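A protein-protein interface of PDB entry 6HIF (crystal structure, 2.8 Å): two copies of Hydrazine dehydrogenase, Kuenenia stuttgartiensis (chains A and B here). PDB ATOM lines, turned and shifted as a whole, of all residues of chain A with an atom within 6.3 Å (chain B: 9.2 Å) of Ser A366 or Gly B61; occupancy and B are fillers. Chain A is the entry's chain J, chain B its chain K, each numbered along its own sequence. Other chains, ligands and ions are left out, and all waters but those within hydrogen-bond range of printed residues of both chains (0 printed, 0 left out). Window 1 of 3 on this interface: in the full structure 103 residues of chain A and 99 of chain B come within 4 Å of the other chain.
The backbone NH of Ser B60 sits at hydrogen-bond distance from the side-chain hydroxyl of Ser A322.
O of Met A323 is in hydrogen-bond range of N of Phe B58.
OH of Tyr B66 sits at hydrogen-bond distance from OD1 of Asp A364, 2.8 Å away.
N of Asp B212 lies within hydrogen-bond range of OD2 of Asp A364, at 3.2 Å.
NZ of Lys A368 lies within salt-bridge range of OD2 of Asp B212 (2.8 Å).
The guanidinium group of Arg A370 is in hydrogen-bond range of the backbone carbonyl oxygen of Gly B61 (2.8 Å).
The backbone carbonyl oxygen of Ala B64 sits at hydrogen-bond distance from the guanidinium group of Arg A370 (3.5 Å).
NE of Arg A370 lies within salt-bridge range of OE2 of Glu B507, at 2.7 Å.
The side-chain carboxylate of Glu A371 lies within hydrogen-bond range of the backbone NH of Glu B507 (3.4 Å).
The backbone NH (N) of Trp B508 sits at hydrogen-bond distance from the side-chain carboxylate (OE1) of Glu A371 (2.8 Å).
The backbone carbonyl oxygen of Gly B46 is in hydrogen-bond range of the side-chain hydroxyl of Tyr A409 (2.8 Å).
The side-chain hydroxyl of Tyr A409 lies within hydrogen-bond range of the backbone NH of Phe B59, 3.2 Å away.
The backbone carbonyl oxygen (O) of Met A323 sits close to the backbone carbonyl oxygen (O) of Lys B56 (3.4 Å).
O of Met A321 sits at hydrogen-bond distance from NE2 of Gln A445 (3.0 Å).
The side-chain amide oxygen (OE1) of Gln A445 lies within hydrogen-bond range of the side-chain hydroxyl (OG) of Ser A366.
The backbone NH (N) of Gly B46 is in hydrogen-bond range of the backbone carbonyl oxygen (O) of Val B57 (2.8 Å).
The side-chain carboxylate of Glu B50 lies within salt-bridge range of the side-chain amino group of Lys B56, at 2.9 Å.
The backbone NH of Asp B52 lies within hydrogen-bond range of the backbone carbonyl oxygen of Lys B65, 2.9 Å away.
NE1 of Trp B508 is in hydrogen-bond range of OD2 of Asp B212 (3.0 Å).
No position is printed for both chains.
Of the 39 pairs that touch across the chains among the printed residues, none has its exchanged pair printed and touching as well.
Of the printed residues of chain A, Gly B61 touches Met A321 (3.8 Å), Met A323 (3.7 Å), Ser A366 (3.4 Å) and Arg A370 (2.8 Å).
No residue of chain B comes within 4 Å of Ala A365.
Of the printed residues of chain B, Leu A367 touches Tyr B66 (3.6 Å), Glu B507 (3.5 Å) and Trp B508 (3.7 Å).
Of the printed residues of chain B, Lys A368 touches Asp B212 (2.8 Å) and Trp B508 (3.5 Å).
Printed residues of chain B within 4 Å of Lys A363: Asp B52 (3.9 Å).
The nearest residue of chain B that does not touch Ser A366 is Ser B60 (4.4 Å).
The nearest residue of chain A that does not touch Gly B61 is Ser A322 (4.1 Å).
The nearest printed residue of chain A that does not touch Gly B46 is Met A323 (7.1 Å).
Ser B60 touches Met A321.
Met A321 touches Gly B61 (O to N, 3.8 Å).
Ser A322 touches Phe B58.
CE of Met A323 touches CB of Asp B52 (3.6 Å).
CB of Met A323 touches CA of Gly B61 (3.7 Å).
OD2 of Asp B52 touches CD of Lys A363, 3.9 Å away.
Tyr B66 touches Leu A367 (CG to CD1, 3.6 Å).
Glu B507 touches Leu A367 (O to CD1, 3.5 Å).
O of Val B57 touches OH of Tyr A409, 3.99 Å away.
Leu B62 touches Tyr A409.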
ATOM      1  N   GLY A 320      11.613  -9.734  -9.003  1.00  0.00           N
ATOM      2  CA  GLY A 320      10.817  -8.841  -9.826  1.00  0.00           C
ATOM      3  C   GLY A 320      10.727  -7.436  -9.233  1.00  0.00           C
ATOM      4  O   GLY A 320      10.009  -6.587  -9.761  1.00  0.00           O
ATOM      5  N   MET A 321      11.468  -7.210  -8.139  1.00  0.00           N
ATOM      6  CA  MET A 321      11.550  -5.909  -7.499  1.00  0.00           C
ATOM      7  C   MET A 321      12.429  -4.988  -8.337  1.00  0.00           C
ATOM      8  O   MET A 321      12.100  -3.819  -8.520  1.00  0.00           O
ATOM      9  CB  MET A 321      12.109  -6.010  -6.077  1.00  0.00           C
ATOM     10  CG  MET A 321      11.197  -6.773  -5.135  1.00  0.00           C
ATOM     11  SD  MET A 321      11.696  -6.739  -3.395  1.00  0.00           S
ATOM     12  CE  MET A 321      13.313  -7.503  -3.484  1.00  0.00           C
ATOM     13  N   SER A 322      13.538  -5.535  -8.848  1.00  0.00           N
ATOM     14  CA  SER A 322      14.332  -4.853  -9.859  1.00  0.00           C
ATOM     15  C   SER A 322      13.641  -4.968 -11.217  1.00  0.00           C
ATOM     16  O   SER A 322      12.869  -5.894 -11.447  1.00  0.00           O
ATOM     17  CB  SER A 322      15.741  -5.383  -9.900  1.00  0.00           C
ATOM     18  OG  SER A 322      16.419  -5.107  -8.681  1.00  0.00           O
ATOM     19  N   MET A 323      13.932  -4.020 -12.110  1.00  0.00           N
ATOM     20  CA  MET A 323      13.188  -3.880 -13.350  1.00  0.00           C
ATOM     21  C   MET A 323      14.116  -4.071 -14.550  1.00  0.00           C
ATOM     22  O   MET A 323      15.250  -3.596 -14.555  1.00  0.00           O
ATOM     23  CB  MET A 323      12.521  -2.501 -13.403  1.00  0.00           C
ATOM     24  CG  MET A 323      11.589  -2.308 -14.579  1.00  0.00           C
ATOM     25  SD  MET A 323      12.439  -1.555 -15.985  1.00  0.00           S
ATOM     26  CE  MET A 323      12.623   0.126 -15.384  1.00  0.00           C
ATOM     27  N   SER A 361       3.999  -3.556 -18.594  1.00  0.00           N
ATOM     28  CA  SER A 361       3.411  -3.477 -17.265  1.00  0.00           C
ATOM     29  C   SER A 361       4.508  -3.314 -16.220  1.00  0.00           C
ATOM     30  O   SER A 361       4.336  -2.582 -15.249  1.00  0.00           O
ATOM     31  CB  SER A 361       2.572  -4.686 -16.974  1.00  0.00           C
ATOM     32  OG  SER A 361       1.519  -4.796 -17.915  1.00  0.00           O
ATOM     33  N   VAL A 362       5.629  -4.007 -16.447  1.00  0.00           N
ATOM     34  CA  VAL A 362       6.762  -4.006 -15.537  1.00  0.00           C
ATOM     35  C   VAL A 362       7.406  -2.618 -15.522  1.00  0.00           C
ATOM     36  O   VAL A 362       7.767  -2.114 -14.457  1.00  0.00           O
ATOM     37  CB  VAL A 362       7.760  -5.120 -15.910  1.00  0.00           C
ATOM     38  CG1 VAL A 362       9.123  -4.932 -15.262  1.00  0.00           C
ATOM     39  CG2 VAL A 362       7.199  -6.491 -15.572  1.00  0.00           C
ATOM     40  N   LYS A 363       7.526  -2.010 -16.708  1.00  0.00           N
ATOM     41  CA  LYS A 363       8.154  -0.707 -16.863  1.00  0.00           C
ATOM     42  C   LYS A 363       7.280   0.385 -16.248  1.00  0.00           C
ATOM     43  O   LYS A 363       7.793   1.294 -15.597  1.00  0.00           O
ATOM     44  CB  LYS A 363       8.450  -0.434 -18.342  1.00  0.00           C
ATOM     45  CG  LYS A 363       9.690  -1.128 -18.888  1.00  0.00           C
ATOM     46  CD  LYS A 363      10.039  -0.726 -20.302  1.00  0.00           C
ATOM     47  CE  LYS A 363       9.110  -1.305 -21.348  1.00  0.00           C
ATOM     48  NZ  LYS A 363       9.466  -0.841 -22.708  1.00  0.00           N
ATOM     49  N   ASP A 364       5.961   0.276 -16.459  1.00  0.00           N
ATOM     50  CA  ASP A 364       5.004   1.249 -15.964  1.00  0.00           C
ATOM     51  C   ASP A 364       4.898   1.163 -14.443  1.00  0.00           C
ATOM     52  O   ASP A 364       4.582   2.154 -13.788  1.00  0.00           O
ATOM     53  CB  ASP A 364       3.640   1.082 -16.639  1.00  0.00           C
ATOM     54  CG  ASP A 364       3.630   1.473 -18.108  1.00  0.00           C
ATOM     55  OD1 ASP A 364       4.646   2.018 -18.582  1.00  0.00           O
ATOM     56  OD2 ASP A 364       2.606   1.221 -18.771  1.00  0.00           O
ATOM     57  N   ALA A 365       5.166  -0.028 -13.894  1.00  0.00           N
ATOM     58  CA  ALA A 365       5.114  -0.257 -12.460  1.00  0.00           C
ATOM     59  C   ALA A 365       6.266   0.468 -11.773  1.00  0.00           C
ATOM     60  O   ALA A 365       6.075   1.063 -10.714  1.00  0.00           O
ATOM     61  CB  ALA A 365       5.149  -1.736 -12.170  1.00  0.00           C
ATOM     62  N   SER A 366       7.456   0.412 -12.389  1.00  0.00           N
ATOM     63  CA  SER A 366       8.652   1.030 -11.833  1.00  0.00           C
ATOM     64  C   SER A 366       8.597   2.551 -11.966  1.00  0.00           C
ATOM     65  O   SER A 366       9.179   3.260 -11.150  1.00  0.00           O
ATOM     66  CB  SER A 366       9.902   0.452 -12.430  1.00  0.00           C
ATOM     67  OG  SER A 366      10.242  -0.757 -11.768  1.00  0.00           O
ATOM     68  N   LEU A 367       7.884   3.036 -12.991  1.00  0.00           N
ATOM     69  CA  LEU A 367       7.583   4.452 -13.129  1.00  0.00           C
ATOM     70  C   LEU A 367       6.871   4.945 -11.872  1.00  0.00           C
ATOM     71  O   LEU A 367       7.235   5.985 -11.325  1.00  0.00           O
ATOM     72  CB  LEU A 367       6.704   4.654 -14.366  1.00  0.00           C
ATOM     73  CG  LEU A 367       6.257   6.090 -14.638  1.00  0.00           C
ATOM     74  CD1 LEU A 367       7.426   6.952 -15.091  1.00  0.00           C
ATOM     75  CD2 LEU A 367       5.155   6.115 -15.684  1.00  0.00           C
ATOM     76  N   LYS A 368       5.866   4.181 -11.423  1.00  0.00           N
ATOM     77  CA  LYS A 368       5.092   4.511 -10.238  1.00  0.00           C
ATOM     78  C   LYS A 368       5.984   4.491  -9.004  1.00  0.00           C
ATOM     79  O   LYS A 368       5.876   5.376  -8.158  1.00  0.00           O
ATOM     80  CB  LYS A 368       3.952   3.513 -10.030  1.00  0.00           C
ATOM     81  CG  LYS A 368       2.580   3.976 -10.491  1.00  0.00           C
ATOM     82  CD  LYS A 368       1.544   2.897 -10.305  1.00  0.00           C
ATOM     83  CE  LYS A 368       0.492   2.926 -11.390  1.00  0.00           C
ATOM     84  NZ  LYS A 368       0.091   1.556 -11.780  1.00  0.00           N
ATOM     85  N   TYR A 369       6.838   3.468  -8.895  1.00  0.00           N
ATOM     86  CA  TYR A 369       7.637   3.309  -7.692  1.00  0.00           C
ATOM     87  C   TYR A 369       8.686   4.414  -7.601  1.00  0.00           C
ATOM     88  O   TYR A 369       8.996   4.884  -6.509  1.00  0.00           O
ATOM     89  CB  TYR A 369       8.253   1.914  -7.583  1.00  0.00           C
ATOM     90  CG  TYR A 369       9.011   1.703  -6.298  1.00  0.00           C
ATOM     91  CD1 TYR A 369       8.352   1.635  -5.081  1.00  0.00           C
ATOM     92  CD2 TYR A 369      10.393   1.599  -6.296  1.00  0.00           C
ATOM     93  CE1 TYR A 369       9.046   1.466  -3.893  1.00  0.00           C
ATOM     94  CE2 TYR A 369      11.101   1.423  -5.119  1.00  0.00           C
ATOM     95  CZ  TYR A 369      10.424   1.353  -3.914  1.00  0.00           C
ATOM     96  OH  TYR A 369      11.129   1.171  -2.759  1.00  0.00           O
ATOM     97  N   ARG A 370       9.216   4.830  -8.761  1.00  0.00           N
ATOM     98  CA  ARG A 370      10.178   5.920  -8.809  1.00  0.00           C
ATOM     99  C   ARG A 370       9.549   7.168  -8.192  1.00  0.00           C
ATOM    100  O   ARG A 370      10.198   7.867  -7.412  1.00  0.00           O
ATOM    101  CB  ARG A 370      10.694   6.143 -10.236  1.00  0.00           C
ATOM    102  CG  ARG A 370      11.827   5.207 -10.632  1.00  0.00           C
ATOM    103  CD  ARG A 370      12.525   5.592 -11.924  1.00  0.00           C
ATOM    104  NE  ARG A 370      11.641   5.599 -13.081  1.00  0.00           N
ATOM    105  CZ  ARG A 370      11.421   4.554 -13.874  1.00  0.00           C
ATOM    106  NH1 ARG A 370      12.030   3.406 -13.639  1.00  0.00           N
ATOM    107  NH2 ARG A 370      10.587   4.655 -14.897  1.00  0.00           N
ATOM    108  N   GLU A 371       8.273   7.412  -8.522  1.00  0.00           N
ATOM    109  CA  GLU A 371       7.532   8.530  -7.960  1.00  0.00           C
ATOM    110  C   GLU A 371       7.359   8.324  -6.458  1.00  0.00           C
ATOM    111  O   GLU A 371       7.487   9.273  -5.685  1.00  0.00           O
ATOM    112  CB  GLU A 371       6.184   8.732  -8.654  1.00  0.00           C
ATOM    113  CG  GLU A 371       5.499  10.022  -8.234  1.00  0.00           C
ATOM    114  CD  GLU A 371       4.142  10.327  -8.849  1.00  0.00           C
ATOM    115  OE1 GLU A 371       3.937  10.005 -10.041  1.00  0.00           O
ATOM    116  OE2 GLU A 371       3.292  10.895  -8.131  1.00  0.00           O
ATOM    117  N   TYR A 409      23.311   3.082  -5.968  1.00  0.00           N
ATOM    118  CA  TYR A 409      22.666   4.280  -6.487  1.00  0.00           C
ATOM    119  C   TYR A 409      22.769   5.443  -5.503  1.00  0.00           C
ATOM    120  O   TYR A 409      22.715   6.604  -5.908  1.00  0.00           O
ATOM    121  CB  TYR A 409      21.185   4.028  -6.796  1.00  0.00           C
ATOM    122  CG  TYR A 409      20.892   3.151  -7.989  1.00  0.00           C
ATOM    123  CD1 TYR A 409      21.807   3.005  -9.021  1.00  0.00           C
ATOM    124  CD2 TYR A 409      19.678   2.489  -8.105  1.00  0.00           C
ATOM    125  CE1 TYR A 409      21.539   2.204 -10.121  1.00  0.00           C
ATOM    126  CE2 TYR A 409      19.390   1.691  -9.201  1.00  0.00           C
ATOM    127  CZ  TYR A 409      20.326   1.545 -10.212  1.00  0.00           C
ATOM    128  OH  TYR A 409      20.061   0.756 -11.294  1.00  0.00           O
ATOM    129  N   VAL A 441       6.987  -2.130  -3.749  1.00  0.00           N
ATOM    130  CA  VAL A 441       7.908  -2.746  -4.691  1.00  0.00           C
ATOM    131  C   VAL A 441       8.060  -4.233  -4.366  1.00  0.00           C
ATOM    132  O   VAL A 441       8.239  -5.047  -5.269  1.00  0.00           O
ATOM    133  CB  VAL A 441       9.264  -2.007  -4.735  1.00  0.00           C
ATOM    134  CG1 VAL A 441      10.073  -2.180  -3.457  1.00  0.00           C
ATOM    135  CG2 VAL A 441      10.096  -2.391  -5.952  1.00  0.00           C
ATOM    136  N   GLN A 445       4.345  -4.796  -6.668  1.00  0.00           N
ATOM    137  CA  GLN A 445       5.031  -4.780  -7.950  1.00  0.00           C
ATOM    138  C   GLN A 445       5.246  -6.207  -8.445  1.00  0.00           C
ATOM    139  O   GLN A 445       5.179  -6.453  -9.647  1.00  0.00           O
ATOM    140  CB  GLN A 445       6.362  -4.031  -7.854  1.00  0.00           C
ATOM    141  CG  GLN A 445       6.846  -3.482  -9.189  1.00  0.00           C
ATOM    142  CD  GLN A 445       8.283  -3.018  -9.157  1.00  0.00           C
ATOM    143  OE1 GLN A 445       8.579  -1.822  -9.083  1.00  0.00           O
ATOM    144  NE2 GLN A 445       9.197  -3.974  -9.213  1.00  0.00           N
ATOM    145  N   MET A 469      -0.253  -0.403  -5.997  1.00  0.00           N
ATOM    146  CA  MET A 469       0.834   0.559  -5.970  1.00  0.00           C
ATOM    147  C   MET A 469       0.265   1.976  -5.959  1.00  0.00           C
ATOM    148  O   MET A 469       0.831   2.858  -5.315  1.00  0.00           O
ATOM    149  CB  MET A 469       1.741   0.389  -7.192  1.00  0.00           C
ATOM    150  CG  MET A 469       2.425  -0.960  -7.253  1.00  0.00           C
ATOM    151  SD  MET A 469       3.691  -1.022  -8.540  1.00  0.00           S
ATOM    152  CE  MET A 469       5.040  -0.173  -7.715  1.00  0.00           C
ATOM    153  N   ILE B  35      17.514  -5.781  -2.002  1.00  0.00           N
ATOM    154  CA  ILE B  35      17.642  -5.468  -3.417  1.00  0.00           C
ATOM    155  C   ILE B  35      19.043  -5.900  -3.849  1.00  0.00           C
ATOM    156  O   ILE B  35      20.011  -5.165  -3.657  1.00  0.00           O
ATOM    157  CB  ILE B  35      17.376  -3.971  -3.690  1.00  0.00           C
ATOM    158  CG1 ILE B  35      16.036  -3.502  -3.115  1.00  0.00           C
ATOM    159  CG2 ILE B  35      17.498  -3.651  -5.175  1.00  0.00           C
ATOM    160  CD1 ILE B  35      14.818  -3.998  -3.866  1.00  0.00           C
ATOM    161  N   GLY B  46      21.908  -1.184 -15.113  1.00  0.00           N
ATOM    162  CA  GLY B  46      21.531   0.136 -15.587  1.00  0.00           C
ATOM    163  C   GLY B  46      21.989   1.211 -14.609  1.00  0.00           C
ATOM    164  O   GLY B  46      21.855   1.048 -13.396  1.00  0.00           O
ATOM    165  N   GLU B  50      19.866   6.222 -17.860  1.00  0.00           N
ATOM    166  CA  GLU B  50      19.827   5.300 -18.986  1.00  0.00           C
ATOM    167  C   GLU B  50      18.382   4.904 -19.295  1.00  0.00           C
ATOM    168  O   GLU B  50      17.532   4.908 -18.404  1.00  0.00           O
ATOM    169  CB  GLU B  50      20.675   4.060 -18.698  1.00  0.00           C
ATOM    170  CG  GLU B  50      22.170   4.306 -18.770  1.00  0.00           C
ATOM    171  CD  GLU B  50      22.985   3.024 -18.745  1.00  0.00           C
ATOM    172  OE1 GLU B  50      22.971   2.293 -19.760  1.00  0.00           O
ATOM    173  OE2 GLU B  50      23.612   2.744 -17.704  1.00  0.00           O
ATOM    174  N   ASP B  52      14.942   2.840 -19.890  1.00  0.00           N
ATOM    175  CA  ASP B  52      14.376   1.694 -19.194  1.00  0.00           C
ATOM    176  C   ASP B  52      14.175   0.534 -20.169  1.00  0.00           C
ATOM    177  O   ASP B  52      14.081  -0.617 -19.752  1.00  0.00           O
ATOM    178  CB  ASP B  52      13.107   2.072 -18.420  1.00  0.00           C
ATOM    179  CG  ASP B  52      11.958   2.577 -19.280  1.00  0.00           C
ATOM    180  OD1 ASP B  52      12.176   2.823 -20.484  1.00  0.00           O
ATOM    181  OD2 ASP B  52      10.847   2.725 -18.736  1.00  0.00           O
ATOM    182  N   LYS B  56      18.555  -3.333 -19.451  1.00  0.00           N
ATOM    183  CA  LYS B  56      19.468  -3.398 -18.323  1.00  0.00           C
ATOM    184  C   LYS B  56      18.659  -3.475 -17.031  1.00  0.00           C
ATOM    185  O   LYS B  56      17.501  -3.068 -16.986  1.00  0.00           O
ATOM    186  CB  LYS B  56      20.451  -2.225 -18.371  1.00  0.00           C
ATOM    187  CG  LYS B  56      21.293  -2.166 -19.637  1.00  0.00           C
ATOM    188  CD  LYS B  56      22.242  -0.992 -19.697  1.00  0.00           C
ATOM    189  CE  LYS B  56      23.627  -1.328 -19.190  1.00  0.00           C
ATOM    190  NZ  LYS B  56      24.498  -0.128 -19.161  1.00  0.00           N
ATOM    191  N   VAL B  57      19.287  -4.022 -15.986  1.00  0.00           N
ATOM    192  CA  VAL B  57      18.640  -4.210 -14.700  1.00  0.00           C
ATOM    193  C   VAL B  57      18.780  -2.920 -13.897  1.00  0.00           C
ATOM    194  O   VAL B  57      19.893  -2.468 -13.638  1.00  0.00           O
ATOM    195  CB  VAL B  57      19.239  -5.409 -13.940  1.00  0.00           C
ATOM    196  CG1 VAL B  57      18.475  -5.692 -12.660  1.00  0.00           C
ATOM    197  CG2 VAL B  57      19.310  -6.658 -14.805  1.00  0.00           C
ATOM    198  N   PHE B  58      17.639  -2.337 -13.517  1.00  0.00           N
ATOM    199  CA  PHE B  58      17.618  -1.177 -12.642  1.00  0.00           C
ATOM    200  C   PHE B  58      17.161  -1.625 -11.259  1.00  0.00           C
ATOM    201  O   PHE B  58      16.040  -2.094 -11.098  1.00  0.00           O
ATOM    202  CB  PHE B  58      16.731  -0.075 -13.224  1.00  0.00           C
ATOM    203  CG  PHE B  58      17.238   0.506 -14.520  1.00  0.00           C
ATOM    204  CD1 PHE B  58      18.102   1.590 -14.521  1.00  0.00           C
ATOM    205  CD2 PHE B  58      16.865  -0.040 -15.741  1.00  0.00           C
ATOM    206  CE1 PHE B  58      18.575   2.120 -15.714  1.00  0.00           C
ATOM    207  CE2 PHE B  58      17.343   0.487 -16.933  1.00  0.00           C
ATOM    208  CZ  PHE B  58      18.196   1.568 -16.918  1.00  0.00           C
ATOM    209  N   PHE B  59      18.055  -1.489 -10.275  1.00  0.00           N
ATOM    210  CA  PHE B  59      17.819  -1.991  -8.931  1.00  0.00           C
ATOM    211  C   PHE B  59      16.595  -1.308  -8.328  1.00  0.00           C
ATOM    212  O   PHE B  59      16.533  -0.081  -8.258  1.00  0.00           O
ATOM    213  CB  PHE B  59      19.075  -1.823  -8.073  1.00  0.00           C
ATOM    214  CG  PHE B  59      20.318  -2.437  -8.664  1.00  0.00           C
ATOM    215  CD1 PHE B  59      20.381  -3.798  -8.940  1.00  0.00           C
ATOM    216  CD2 PHE B  59      21.429  -1.657  -8.949  1.00  0.00           C
ATOM    217  CE1 PHE B  59      21.522  -4.364  -9.490  1.00  0.00           C
ATOM    218  CE2 PHE B  59      22.572  -2.227  -9.493  1.00  0.00           C
ATOM    219  CZ  PHE B  59      22.618  -3.577  -9.761  1.00  0.00           C
ATOM    220  N   SER B  60      15.623  -2.128  -7.915  1.00  0.00           N
ATOM    221  CA  SER B  60      14.359  -1.663  -7.363  1.00  0.00           C
ATOM    222  C   SER B  60      13.601  -0.799  -8.374  1.00  0.00           C
ATOM    223  O   SER B  60      12.596  -0.174  -8.040  1.00  0.00           O
ATOM    224  CB  SER B  60      14.555  -0.956  -6.050  1.00  0.00           C
ATOM    225  OG  SER B  60      13.325  -0.858  -5.353  1.00  0.00           O
ATOM    226  N   GLY B  61      14.083  -0.787  -9.620  1.00  0.00           N
ATOM    227  CA  GLY B  61      13.424  -0.077 -10.703  1.00  0.00           C
ATOM    228  C   GLY B  61      13.724   1.419 -10.682  1.00  0.00           C
ATOM    229  O   GLY B  61      13.033   2.197 -11.337  1.00  0.00           O
ATOM    230  N   LEU B  62      14.774   1.803  -9.946  1.00  0.00           N
ATOM    231  CA  LEU B  62      15.096   3.203  -9.723  1.00  0.00           C
ATOM    232  C   LEU B  62      16.040   3.717 -10.808  1.00  0.00           C
ATOM    233  O   LEU B  62      16.734   2.940 -11.462  1.00  0.00           O
ATOM    234  CB  LEU B  62      15.727   3.356  -8.334  1.00  0.00           C
ATOM    235  CG  LEU B  62      14.816   3.051  -7.145  1.00  0.00           C
ATOM    236  CD1 LEU B  62      15.526   3.346  -5.835  1.00  0.00           C
ATOM    237  CD2 LEU B  62      13.517   3.837  -7.226  1.00  0.00           C
ATOM    238  N   LYS B  63      16.020   5.044 -11.000  1.00  0.00           N
ATOM    239  CA  LYS B  63      17.069   5.800 -11.671  1.00  0.00           C
ATOM    240  C   LYS B  63      16.995   5.654 -13.193  1.00  0.00           C
ATOM    241  O   LYS B  63      17.813   6.232 -13.907  1.00  0.00           O
ATOM    242  CB  LYS B  63      18.452   5.458 -11.100  1.00  0.00           C
ATOM    243  CG  LYS B  63      18.714   5.942  -9.680  1.00  0.00           C
ATOM    244  CD  LYS B  63      19.012   7.428  -9.593  1.00  0.00           C
ATOM    245  CE  LYS B  63      19.585   7.854  -8.258  1.00  0.00           C
ATOM    246  NZ  LYS B  63      18.538   7.939  -7.214  1.00  0.00           N
ATOM    247  N   ALA B  64      16.006   4.904 -13.689  1.00  0.00           N
ATOM    248  CA  ALA B  64      15.859   4.701 -15.122  1.00  0.00           C
ATOM    249  C   ALA B  64      15.114   5.881 -15.748  1.00  0.00           C
ATOM    250  O   ALA B  64      14.323   6.552 -15.086  1.00  0.00           O
ATOM    251  CB  ALA B  64      15.159   3.394 -15.400  1.00  0.00           C
ATOM    252  N   LYS B  65      15.394   6.118 -17.033  1.00  0.00           N
ATOM    253  CA  LYS B  65      14.685   7.105 -17.828  1.00  0.00           C
ATOM    254  C   LYS B  65      13.532   6.403 -18.543  1.00  0.00           C
ATOM    255  O   LYS B  65      13.746   5.466 -19.313  1.00  0.00           O
ATOM    256  CB  LYS B  65      15.658   7.776 -18.804  1.00  0.00           C
ATOM    257  CG  LYS B  65      15.046   8.725 -19.824  1.00  0.00           C
ATOM    258  CD  LYS B  65      16.072   9.231 -20.817  1.00  0.00           C
ATOM    259  CE  LYS B  65      15.474   9.769 -22.100  1.00  0.00           C
ATOM    260  NZ  LYS B  65      14.769  11.055 -21.884  1.00  0.00           N
ATOM    261  N   TYR B  66      12.308   6.861 -18.258  1.00  0.00           N
ATOM    262  CA  TYR B  66      11.100   6.249 -18.786  1.00  0.00           C
ATOM    263  C   TYR B  66      10.959   6.603 -20.262  1.00  0.00           C
ATOM    264  O   TYR B  66      10.886   7.779 -20.610  1.00  0.00           O
ATOM    265  CB  TYR B  66       9.882   6.690 -17.969  1.00  0.00           C
ATOM    266  CG  TYR B  66       8.563   6.115 -18.423  1.00  0.00           C
ATOM    267  CD1 TYR B  66       8.219   4.799 -18.149  1.00  0.00           C
ATOM    268  CD2 TYR B  66       7.650   6.893 -19.115  1.00  0.00           C
ATOM    269  CE1 TYR B  66       7.007   4.268 -18.560  1.00  0.00           C
ATOM    270  CE2 TYR B  66       6.433   6.380 -19.528  1.00  0.00           C
ATOM    271  CZ  TYR B  66       6.111   5.064 -19.252  1.00  0.00           C
ATOM    272  OH  TYR B  66       4.912   4.565 -19.669  1.00  0.00           O
ATOM    273  N   ASP B 212       0.032  -0.372 -17.759  1.00  0.00           N
ATOM    274  CA  ASP B 212      -0.501  -0.059 -16.446  1.00  0.00           C
ATOM    275  C   ASP B 212      -1.821  -0.806 -16.269  1.00  0.00           C
ATOM    276  O   ASP B 212      -2.084  -1.357 -15.204  1.00  0.00           O
ATOM    277  CB  ASP B 212      -0.675   1.453 -16.279  1.00  0.00           C
ATOM    278  CG  ASP B 212      -0.884   1.906 -14.845  1.00  0.00           C
ATOM    279  OD1 ASP B 212      -1.915   1.529 -14.248  1.00  0.00           O
ATOM    280  OD2 ASP B 212      -0.014   2.643 -14.341  1.00  0.00           O
ATOM    281  N   GLU B 507       6.649  11.450 -11.445  1.00  0.00           N
ATOM    282  CA  GLU B 507       7.124  10.732 -12.617  1.00  0.00           C
ATOM    283  C   GLU B 507       5.967  10.025 -13.325  1.00  0.00           C
ATOM    284  O   GLU B 507       5.891  10.044 -14.554  1.00  0.00           O
ATOM    285  CB  GLU B 507       8.272   9.791 -12.253  1.00  0.00           C
ATOM    286  CG  GLU B 507       9.262   9.616 -13.391  1.00  0.00           C
ATOM    287  CD  GLU B 507      10.543   8.888 -13.029  1.00  0.00           C
ATOM    288  OE1 GLU B 507      11.030   9.082 -11.897  1.00  0.00           O
ATOM    289  OE2 GLU B 507      11.051   8.133 -13.884  1.00  0.00           O
ATOM    290  N   TRP B 508       5.065   9.423 -12.538  1.00  0.00           N
ATOM    291  CA  TRP B 508       3.921   8.703 -13.076  1.00  0.00           C
ATOM    292  C   TRP B 508       2.808   9.676 -13.460  1.00  0.00           C
ATOM    293  O   TRP B 508       2.249   9.568 -14.552  1.00  0.00           O
ATOM    294  CB  TRP B 508       3.432   7.623 -12.098  1.00  0.00           C
ATOM    295  CG  TRP B 508       2.217   6.885 -12.575  1.00  0.00           C
ATOM    296  CD1 TRP B 508       2.170   5.909 -13.528  1.00  0.00           C
ATOM    297  CD2 TRP B 508       0.862   7.072 -12.128  1.00  0.00           C
ATOM    298  NE1 TRP B 508       0.883   5.476 -13.707  1.00  0.00           N
ATOM    299  CE2 TRP B 508       0.057   6.172 -12.863  1.00  0.00           C
ATOM    300  CE3 TRP B 508       0.249   7.911 -11.188  1.00  0.00           C
ATOM    301  CZ2 TRP B 508      -1.323   6.091 -12.680  1.00  0.00           C
ATOM    302  CZ3 TRP B 508      -1.115   7.829 -11.005  1.00  0.00           C
ATOM    303  CH2 TRP B 508      -1.888   6.928 -11.741  1.00  0.00           C
